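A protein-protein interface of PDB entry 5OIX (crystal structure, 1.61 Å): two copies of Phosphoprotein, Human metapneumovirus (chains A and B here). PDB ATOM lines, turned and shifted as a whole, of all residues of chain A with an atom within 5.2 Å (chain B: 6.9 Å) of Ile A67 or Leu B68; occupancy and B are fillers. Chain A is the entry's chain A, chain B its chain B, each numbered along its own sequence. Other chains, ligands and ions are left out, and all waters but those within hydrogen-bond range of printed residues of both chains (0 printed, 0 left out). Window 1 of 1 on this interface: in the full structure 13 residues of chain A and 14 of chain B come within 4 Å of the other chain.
Lys A63 touches Ser B65, but with the chains exchanged Ser A65 does not touch Lys B63 (11.8 Å).
Met A66 touches Leu B68, but with the chains exchanged Leu A68 does not touch Met B66 (11.8 Å).
Ile A67 touches Leu B68, but with the chains exchanged Leu A68 does not touch Ile B67 (7.7 Å).
Leu B71 touches its own counterpart, Leu A71.
Positions printed for both chains: 63, 64, 65, 66, 67, 68, 69, 70 and 71.
Of the 11 pairs that touch across the chains among the printed residues, 3 have their exchanged pair printed and touching as well.
Along chain A the printed residues that touch a printed residue of chain B span positions 63 to 71.
Printed residues of chain B that touch a printed residue of chain A: Leu B64, Ser B65, Ile B67, Leu B68, Leu B71 and Arg B72.
Hydrophobic or aromatic side chains of chain B within 4 Å of the printed part of chain A: Leu B64, Ile B67, Leu B68 and Leu B71.
CB of Leu B64 touches CD of Lys A63, at 3.9 Å.
Leu A64 touches Leu B64.
CB of Met A66 touches CD2 of Leu B68 (3.9 Å).
Met A66 touches Arg B72.
Ile A67 touches Leu B64 (CD1 to CD2, 3.6 Å).
Ile A67 touches Ile B67.
Leu B68 touches Ile A67.
Ile A67 touches Leu B71.
CD1 of Leu A70 touches CD2 of Leu B68 (3.8 Å).
CD2 of Leu A71 touches CD2 of Leu B71 (3.7 Å).
OG of Ser B65 lies within hydrogen-bond range of NZ of Lys A63, at 3.3 Å.
Printed residues of chain B within 4 Å of Met A66: Leu B68 and Arg B72.
Of chain B, only Leu B64, Ile B67, Leu B68 and Leu B71 come within 4 Å of Ile A67.
Leu A68 touches none of the printed residues of chain B.
Of the printed residues of chain B, Leu A70 touches Leu B68.
Lys B63 touches none of the printed residues of chain A.
Printed residues of chain A within 4 Å of Leu B64: Lys A63, Leu A64 and Ile A67.
Of the printed residues of chain A, Ser B65 touches Lys A63 (3.3 Å).
Leu B68 touches three residues of chain A.
The nearest residue of chain B that does not touch Ile A67 is Ser B65 (5.8 Å).
The nearest residue of chain A that does not touch Leu B68 is Lys A63 (4.1 Å).
The nearest printed residue of chain A that does not touch Leu B71 is Leu A70 (4.5 Å).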
ATOM      1  N   GLU A  62      -6.500  11.247 -24.976  1.00  0.00           N
ATOM      2  CA  GLU A  62      -7.283  12.099 -24.077  1.00  0.00           C
ATOM      3  C   GLU A  62      -6.741  12.068 -22.655  1.00  0.00           C
ATOM      4  O   GLU A  62      -6.735  13.099 -21.966  1.00  0.00           O
ATOM      5  CB  GLU A  62      -8.761  11.723 -24.127  1.00  0.00           C
ATOM      6  CG  GLU A  62      -9.333  12.103 -25.479  1.00  0.00           C
ATOM      7  CD  GLU A  62     -10.827  11.880 -25.620  1.00  0.00           C
ATOM      8  OE1 GLU A  62     -11.422  11.124 -24.828  1.00  0.00           O
ATOM      9  OE2 GLU A  62     -11.418  12.513 -26.519  1.00  0.00           O
ATOM     10  N   LYS A  63      -6.310  10.901 -22.187  1.00  0.00           N
ATOM     11  CA  LYS A  63      -5.723  10.840 -20.853  1.00  0.00           C
ATOM     12  C   LYS A  63      -4.450  11.669 -20.784  1.00  0.00           C
ATOM     13  O   LYS A  63      -4.184  12.318 -19.762  1.00  0.00           O
ATOM     14  CB  LYS A  63      -5.441   9.389 -20.462  1.00  0.00           C
ATOM     15  CG  LYS A  63      -6.693   8.582 -20.237  1.00  0.00           C
ATOM     16  CD  LYS A  63      -6.373   7.155 -19.805  1.00  0.00           C
ATOM     17  CE  LYS A  63      -7.636   6.330 -19.667  1.00  0.00           C
ATOM     18  NZ  LYS A  63      -8.642   6.960 -18.789  1.00  0.00           N
ATOM     19  N   LEU A  64      -3.639  11.652 -21.853  1.00  0.00           N
ATOM     20  CA  LEU A  64      -2.433  12.484 -21.862  1.00  0.00           C
ATOM     21  C   LEU A  64      -2.765  13.967 -21.778  1.00  0.00           C
ATOM     22  O   LEU A  64      -2.058  14.727 -21.100  1.00  0.00           O
ATOM     23  CB  LEU A  64      -1.609  12.231 -23.121  1.00  0.00           C
ATOM     24  CG  LEU A  64      -0.840  10.921 -23.134  1.00  0.00           C
ATOM     25  CD1 LEU A  64      -0.315  10.669 -24.531  1.00  0.00           C
ATOM     26  CD2 LEU A  64       0.316  10.991 -22.119  1.00  0.00           C
ATOM     27  N   SER A  65      -3.809  14.405 -22.489  1.00  0.00           N
ATOM     28  CA  SER A  65      -4.226  15.803 -22.400  1.00  0.00           C
ATOM     29  C   SER A  65      -4.664  16.171 -20.984  1.00  0.00           C
ATOM     30  O   SER A  65      -4.345  17.261 -20.487  1.00  0.00           O
ATOM     31  CB  SER A  65      -5.342  16.069 -23.409  1.00  0.00           C
ATOM     32  OG  SER A  65      -5.810  17.406 -23.312  1.00  0.00           O
ATOM     33  N   MET A  66      -5.404  15.279 -20.319  1.00  0.00           N
ATOM     34  CA  MET A  66      -5.809  15.533 -18.937  1.00  0.00           C
ATOM     35  C   MET A  66      -4.598  15.611 -18.019  1.00  0.00           C
ATOM     36  O   MET A  66      -4.535  16.473 -17.129  1.00  0.00           O
ATOM     37  CB  MET A  66      -6.752  14.433 -18.450  1.00  0.00           C
ATOM     38  CG  MET A  66      -8.075  14.364 -19.166  1.00  0.00           C
ATOM     39  SD  MET A  66      -8.833  12.747 -18.899  1.00  0.00           S
ATOM     40  CE  MET A  66      -9.420  12.880 -17.217  1.00  0.00           C
ATOM     41  N   ILE A  67      -3.624  14.716 -18.221  1.00  0.00           N
ATOM     42  CA  ILE A  67      -2.427  14.710 -17.376  1.00  0.00           C
ATOM     43  C   ILE A  67      -1.649  16.010 -17.534  1.00  0.00           C
ATOM     44  O   ILE A  67      -1.299  16.670 -16.543  1.00  0.00           O
ATOM     45  CB  ILE A  67      -1.541  13.493 -17.713  1.00  0.00           C
ATOM     46  CG1 ILE A  67      -2.186  12.215 -17.186  1.00  0.00           C
ATOM     47  CG2 ILE A  67      -0.122  13.708 -17.160  1.00  0.00           C
ATOM     48  CD1 ILE A  67      -1.634  10.913 -17.813  1.00  0.00           C
ATOM     49  N   LEU A  68      -1.395  16.412 -18.785  1.00  0.00           N
ATOM     50  CA  LEU A  68      -0.644  17.640 -19.036  1.00  0.00           C
ATOM     51  C   LEU A  68      -1.372  18.844 -18.468  1.00  0.00           C
ATOM     52  O   LEU A  68      -0.741  19.760 -17.923  1.00  0.00           O
ATOM     53  CB  LEU A  68      -0.396  17.822 -20.532  1.00  0.00           C
ATOM     54  CG  LEU A  68       0.768  17.009 -21.092  1.00  0.00           C
ATOM     55  CD1 LEU A  68       0.708  16.951 -22.621  1.00  0.00           C
ATOM     56  CD2 LEU A  68       2.068  17.639 -20.612  1.00  0.00           C
ATOM     57  N   GLY A  69      -2.700  18.865 -18.593  1.00  0.00           N
ATOM     58  CA  GLY A  69      -3.462  19.970 -18.035  1.00  0.00           C
ATOM     59  C   GLY A  69      -3.300  20.073 -16.533  1.00  0.00           C
ATOM     60  O   GLY A  69      -3.185  21.172 -15.984  1.00  0.00           O
ATOM     61  N   LEU A  70      -3.301  18.930 -15.847  1.00  0.00           N
ATOM     62  CA  LEU A  70      -3.111  18.938 -14.402  1.00  0.00           C
ATOM     63  C   LEU A  70      -1.702  19.383 -14.036  1.00  0.00           C
ATOM     64  O   LEU A  70      -1.514  20.114 -13.057  1.00  0.00           O
ATOM     65  CB  LEU A  70      -3.407  17.559 -13.811  1.00  0.00           C
ATOM     66  CG  LEU A  70      -4.873  17.129 -13.777  1.00  0.00           C
ATOM     67  CD1 LEU A  70      -4.987  15.673 -13.384  1.00  0.00           C
ATOM     68  CD2 LEU A  70      -5.654  18.007 -12.806  1.00  0.00           C
ATOM     69  N   LEU A  71      -0.701  18.987 -14.828  1.00  0.00           N
ATOM     70  CA  LEU A  71       0.665  19.383 -14.495  1.00  0.00           C
ATOM     71  C   LEU A  71       0.850  20.896 -14.516  1.00  0.00           C
ATOM     72  O   LEU A  71       1.553  21.446 -13.660  1.00  0.00           O
ATOM     73  CB  LEU A  71       1.660  18.722 -15.444  1.00  0.00           C
ATOM     74  CG  LEU A  71       1.975  17.256 -15.190  1.00  0.00           C
ATOM     75  CD1 LEU A  71       2.867  16.723 -16.308  1.00  0.00           C
ATOM     76  CD2 LEU A  71       2.657  17.139 -13.841  1.00  0.00           C
ATOM     77  N   LYS B  63      -1.878   2.303 -17.167  1.00  0.00           N
ATOM     78  CA  LYS B  63      -0.843   3.069 -16.473  1.00  0.00           C
ATOM     79  C   LYS B  63      -1.166   4.558 -16.476  1.00  0.00           C
ATOM     80  O   LYS B  63      -0.922   5.259 -15.479  1.00  0.00           O
ATOM     81  CB  LYS B  63       0.522   2.795 -17.098  1.00  0.00           C
ATOM     82  CG  LYS B  63       1.021   1.396 -16.769  1.00  0.00           C
ATOM     83  CD  LYS B  63       2.413   1.141 -17.318  1.00  0.00           C
ATOM     84  CE  LYS B  63       2.881  -0.267 -16.952  1.00  0.00           C
ATOM     85  NZ  LYS B  63       1.965  -1.311 -17.477  1.00  0.00           N
ATOM     86  N   LEU B  64      -1.728   5.054 -17.580  1.00  0.00           N
ATOM     87  CA  LEU B  64      -2.112   6.465 -17.648  1.00  0.00           C
ATOM     88  C   LEU B  64      -3.216   6.789 -16.652  1.00  0.00           C
ATOM     89  O   LEU B  64      -3.229   7.883 -16.070  1.00  0.00           O
ATOM     90  CB  LEU B  64      -2.534   6.834 -19.077  1.00  0.00           C
ATOM     91  CG  LEU B  64      -1.361   6.933 -20.057  1.00  0.00           C
ATOM     92  CD1 LEU B  64      -1.889   7.032 -21.519  1.00  0.00           C
ATOM     93  CD2 LEU B  64      -0.411   8.102 -19.741  1.00  0.00           C
ATOM     94  N   SER B  65      -4.177   5.879 -16.476  1.00  0.00           N
ATOM     95  CA  SER B  65      -5.202   6.081 -15.453  1.00  0.00           C
ATOM     96  C   SER B  65      -4.574   6.142 -14.063  1.00  0.00           C
ATOM     97  O   SER B  65      -4.949   6.987 -13.241  1.00  0.00           O
ATOM     98  CB  SER B  65      -6.249   4.969 -15.515  1.00  0.00           C
ATOM     99  OG  SER B  65      -7.013   5.068 -16.708  1.00  0.00           O
ATOM    100  N   MET B  66      -3.589   5.275 -13.796  1.00  0.00           N
ATOM    101  CA  MET B  66      -2.904   5.314 -12.506  1.00  0.00           C
ATOM    102  C   MET B  66      -2.151   6.622 -12.317  1.00  0.00           C
ATOM    103  O   MET B  66      -2.136   7.184 -11.215  1.00  0.00           O
ATOM    104  CB  MET B  66      -1.936   4.128 -12.381  1.00  0.00           C
ATOM    105  CG  MET B  66      -2.546   2.870 -11.765  1.00  0.00           C
ATOM    106  SD  MET B  66      -1.303   1.573 -11.512  1.00  0.00           S
ATOM    107  CE  MET B  66      -0.851   1.297 -13.222  1.00  0.00           C
ATOM    108  N   ILE B  67      -1.473   7.086 -13.368  1.00  0.00           N
ATOM    109  CA  ILE B  67      -0.760   8.365 -13.328  1.00  0.00           C
ATOM    110  C   ILE B  67      -1.721   9.497 -13.003  1.00  0.00           C
ATOM    111  O   ILE B  67      -1.414  10.375 -12.181  1.00  0.00           O
ATOM    112  CB  ILE B  67      -0.018   8.589 -14.660  1.00  0.00           C
ATOM    113  CG1 ILE B  67       1.213   7.679 -14.714  1.00  0.00           C
ATOM    114  CG2 ILE B  67       0.332  10.051 -14.871  1.00  0.00           C
ATOM    115  CD1 ILE B  67       1.771   7.498 -16.136  1.00  0.00           C
ATOM    116  N   LEU B  68      -2.902   9.488 -13.630  1.00  0.00           N
ATOM    117  CA  LEU B  68      -3.900  10.511 -13.313  1.00  0.00           C
ATOM    118  C   LEU B  68      -4.284  10.472 -11.838  1.00  0.00           C
ATOM    119  O   LEU B  68      -4.372  11.524 -11.183  1.00  0.00           O
ATOM    120  CB  LEU B  68      -5.138  10.327 -14.195  1.00  0.00           C
ATOM    121  CG  LEU B  68      -5.053  10.962 -15.574  1.00  0.00           C
ATOM    122  CD1 LEU B  68      -6.137  10.426 -16.506  1.00  0.00           C
ATOM    123  CD2 LEU B  68      -5.182  12.481 -15.407  1.00  0.00           C
ATOM    124  N   GLY B  69      -4.479   9.272 -11.283  1.00  0.00           N
ATOM    125  CA  GLY B  69      -4.809   9.167  -9.866  1.00  0.00           C
ATOM    126  C   GLY B  69      -3.719   9.700  -8.950  1.00  0.00           C
ATOM    127  O   GLY B  69      -4.009  10.337  -7.935  1.00  0.00           O
ATOM    128  N   LEU B  70      -2.455   9.410  -9.271  1.00  0.00           N
ATOM    129  CA  LEU B  70      -1.331   9.877  -8.458  1.00  0.00           C
ATOM    130  C   LEU B  70      -1.185  11.392  -8.545  1.00  0.00           C
ATOM    131  O   LEU B  70      -0.849  12.046  -7.553  1.00  0.00           O
ATOM    132  CB  LEU B  70      -0.055   9.166  -8.912  1.00  0.00           C
ATOM    133  CG  LEU B  70       0.036   7.685  -8.520  1.00  0.00           C
ATOM    134  CD1 LEU B  70       1.120   6.949  -9.343  1.00  0.00           C
ATOM    135  CD2 LEU B  70       0.355   7.597  -7.007  1.00  0.00           C
ATOM    136  N   LEU B  71      -1.409  11.964  -9.738  1.00  0.00           N
ATOM    137  CA  LEU B  71      -1.358  13.419  -9.884  1.00  0.00           C
ATOM    138  C   LEU B  71      -2.478  14.105  -9.120  1.00  0.00           C
ATOM    139  O   LEU B  71      -2.268  15.182  -8.539  1.00  0.00           O
ATOM    140  CB  LEU B  71      -1.421  13.822 -11.356  1.00  0.00           C
ATOM    141  CG  LEU B  71      -0.139  13.711 -12.148  1.00  0.00           C
ATOM    142  CD1 LEU B  71      -0.415  13.979 -13.613  1.00  0.00           C
ATOM    143  CD2 LEU B  71       0.830  14.764 -11.587  1.00  0.00           C
ATOM    144  N   ARG B  72      -3.677  13.513  -9.119  1.00  0.00           N
ATOM    145  CA  ARG B  72      -4.791  14.117  -8.388  1.00  0.00           C
ATOM    146  C   ARG B  72      -4.522  14.131  -6.887  1.00  0.00           C
ATOM    147  O   ARG B  72      -4.825  15.117  -6.205  1.00  0.00           O
ATOM    148  CB  ARG B  72      -6.089  13.375  -8.717  1.00  0.00           C
ATOM    149  CG  ARG B  72      -6.585  13.647 -10.138  1.00  0.00           C
ATOM    150  CD  ARG B  72      -7.834  12.845 -10.513  1.00  0.00           C
ATOM    151  NE  ARG B  72      -8.286  13.158 -11.869  1.00  0.00           N
ATOM    152  CZ  ARG B  72      -9.095  12.389 -12.595  1.00  0.00           C
ATOM    153  NH1 ARG B  72      -9.542  11.240 -12.110  1.00  0.00           N
ATOM    154  NH2 ARG B  72      -9.447  12.765 -13.819  1.00  0.00           N
ATOM    155  N   THR B  73      -3.933  13.060  -6.353  1.00  0.00           N
ATOM    156  CA  THR B  73      -3.561  13.025  -4.942  1.00  0.00           C
ATOM    157  C   THR B  73      -2.458  14.027  -4.632  1.00  0.00           C
ATOM    158  O   THR B  73      -2.416  14.601  -3.539  1.00  0.00           O
ATOM    159  CB  THR B  73      -3.114  11.610  -4.575  1.00  0.00           C
ATOM    160  OG1 THR B  73      -4.110  10.677  -5.013  1.00  0.00           O
ATOM    161  CG2 THR B  73      -2.904  11.457  -3.084  1.00  0.00           C
ATOM    162  N   LEU B  74      -1.546  14.236  -5.582  1.00  0.00           N
ATOM    163  CA  LEU B  74      -0.418  15.123  -5.329  1.00  0.00           C
ATOM    164  C   LEU B  74      -0.867  16.572  -5.247  1.00  0.00           C
ATOM    165  O   LEU B  74      -0.207  17.385  -4.589  1.00  0.00           O
ATOM    166  CB  LEU B  74       0.628  14.951  -6.432  1.00  0.00           C
ATOM    167  CG  LEU B  74       1.998  15.611  -6.305  1.00  0.00           C
ATOM    168  CD1 LEU B  74       2.683  15.118  -5.048  1.00  0.00           C
ATOM    169  CD2 LEU B  74       2.849  15.321  -7.530  1.00  0.00           C
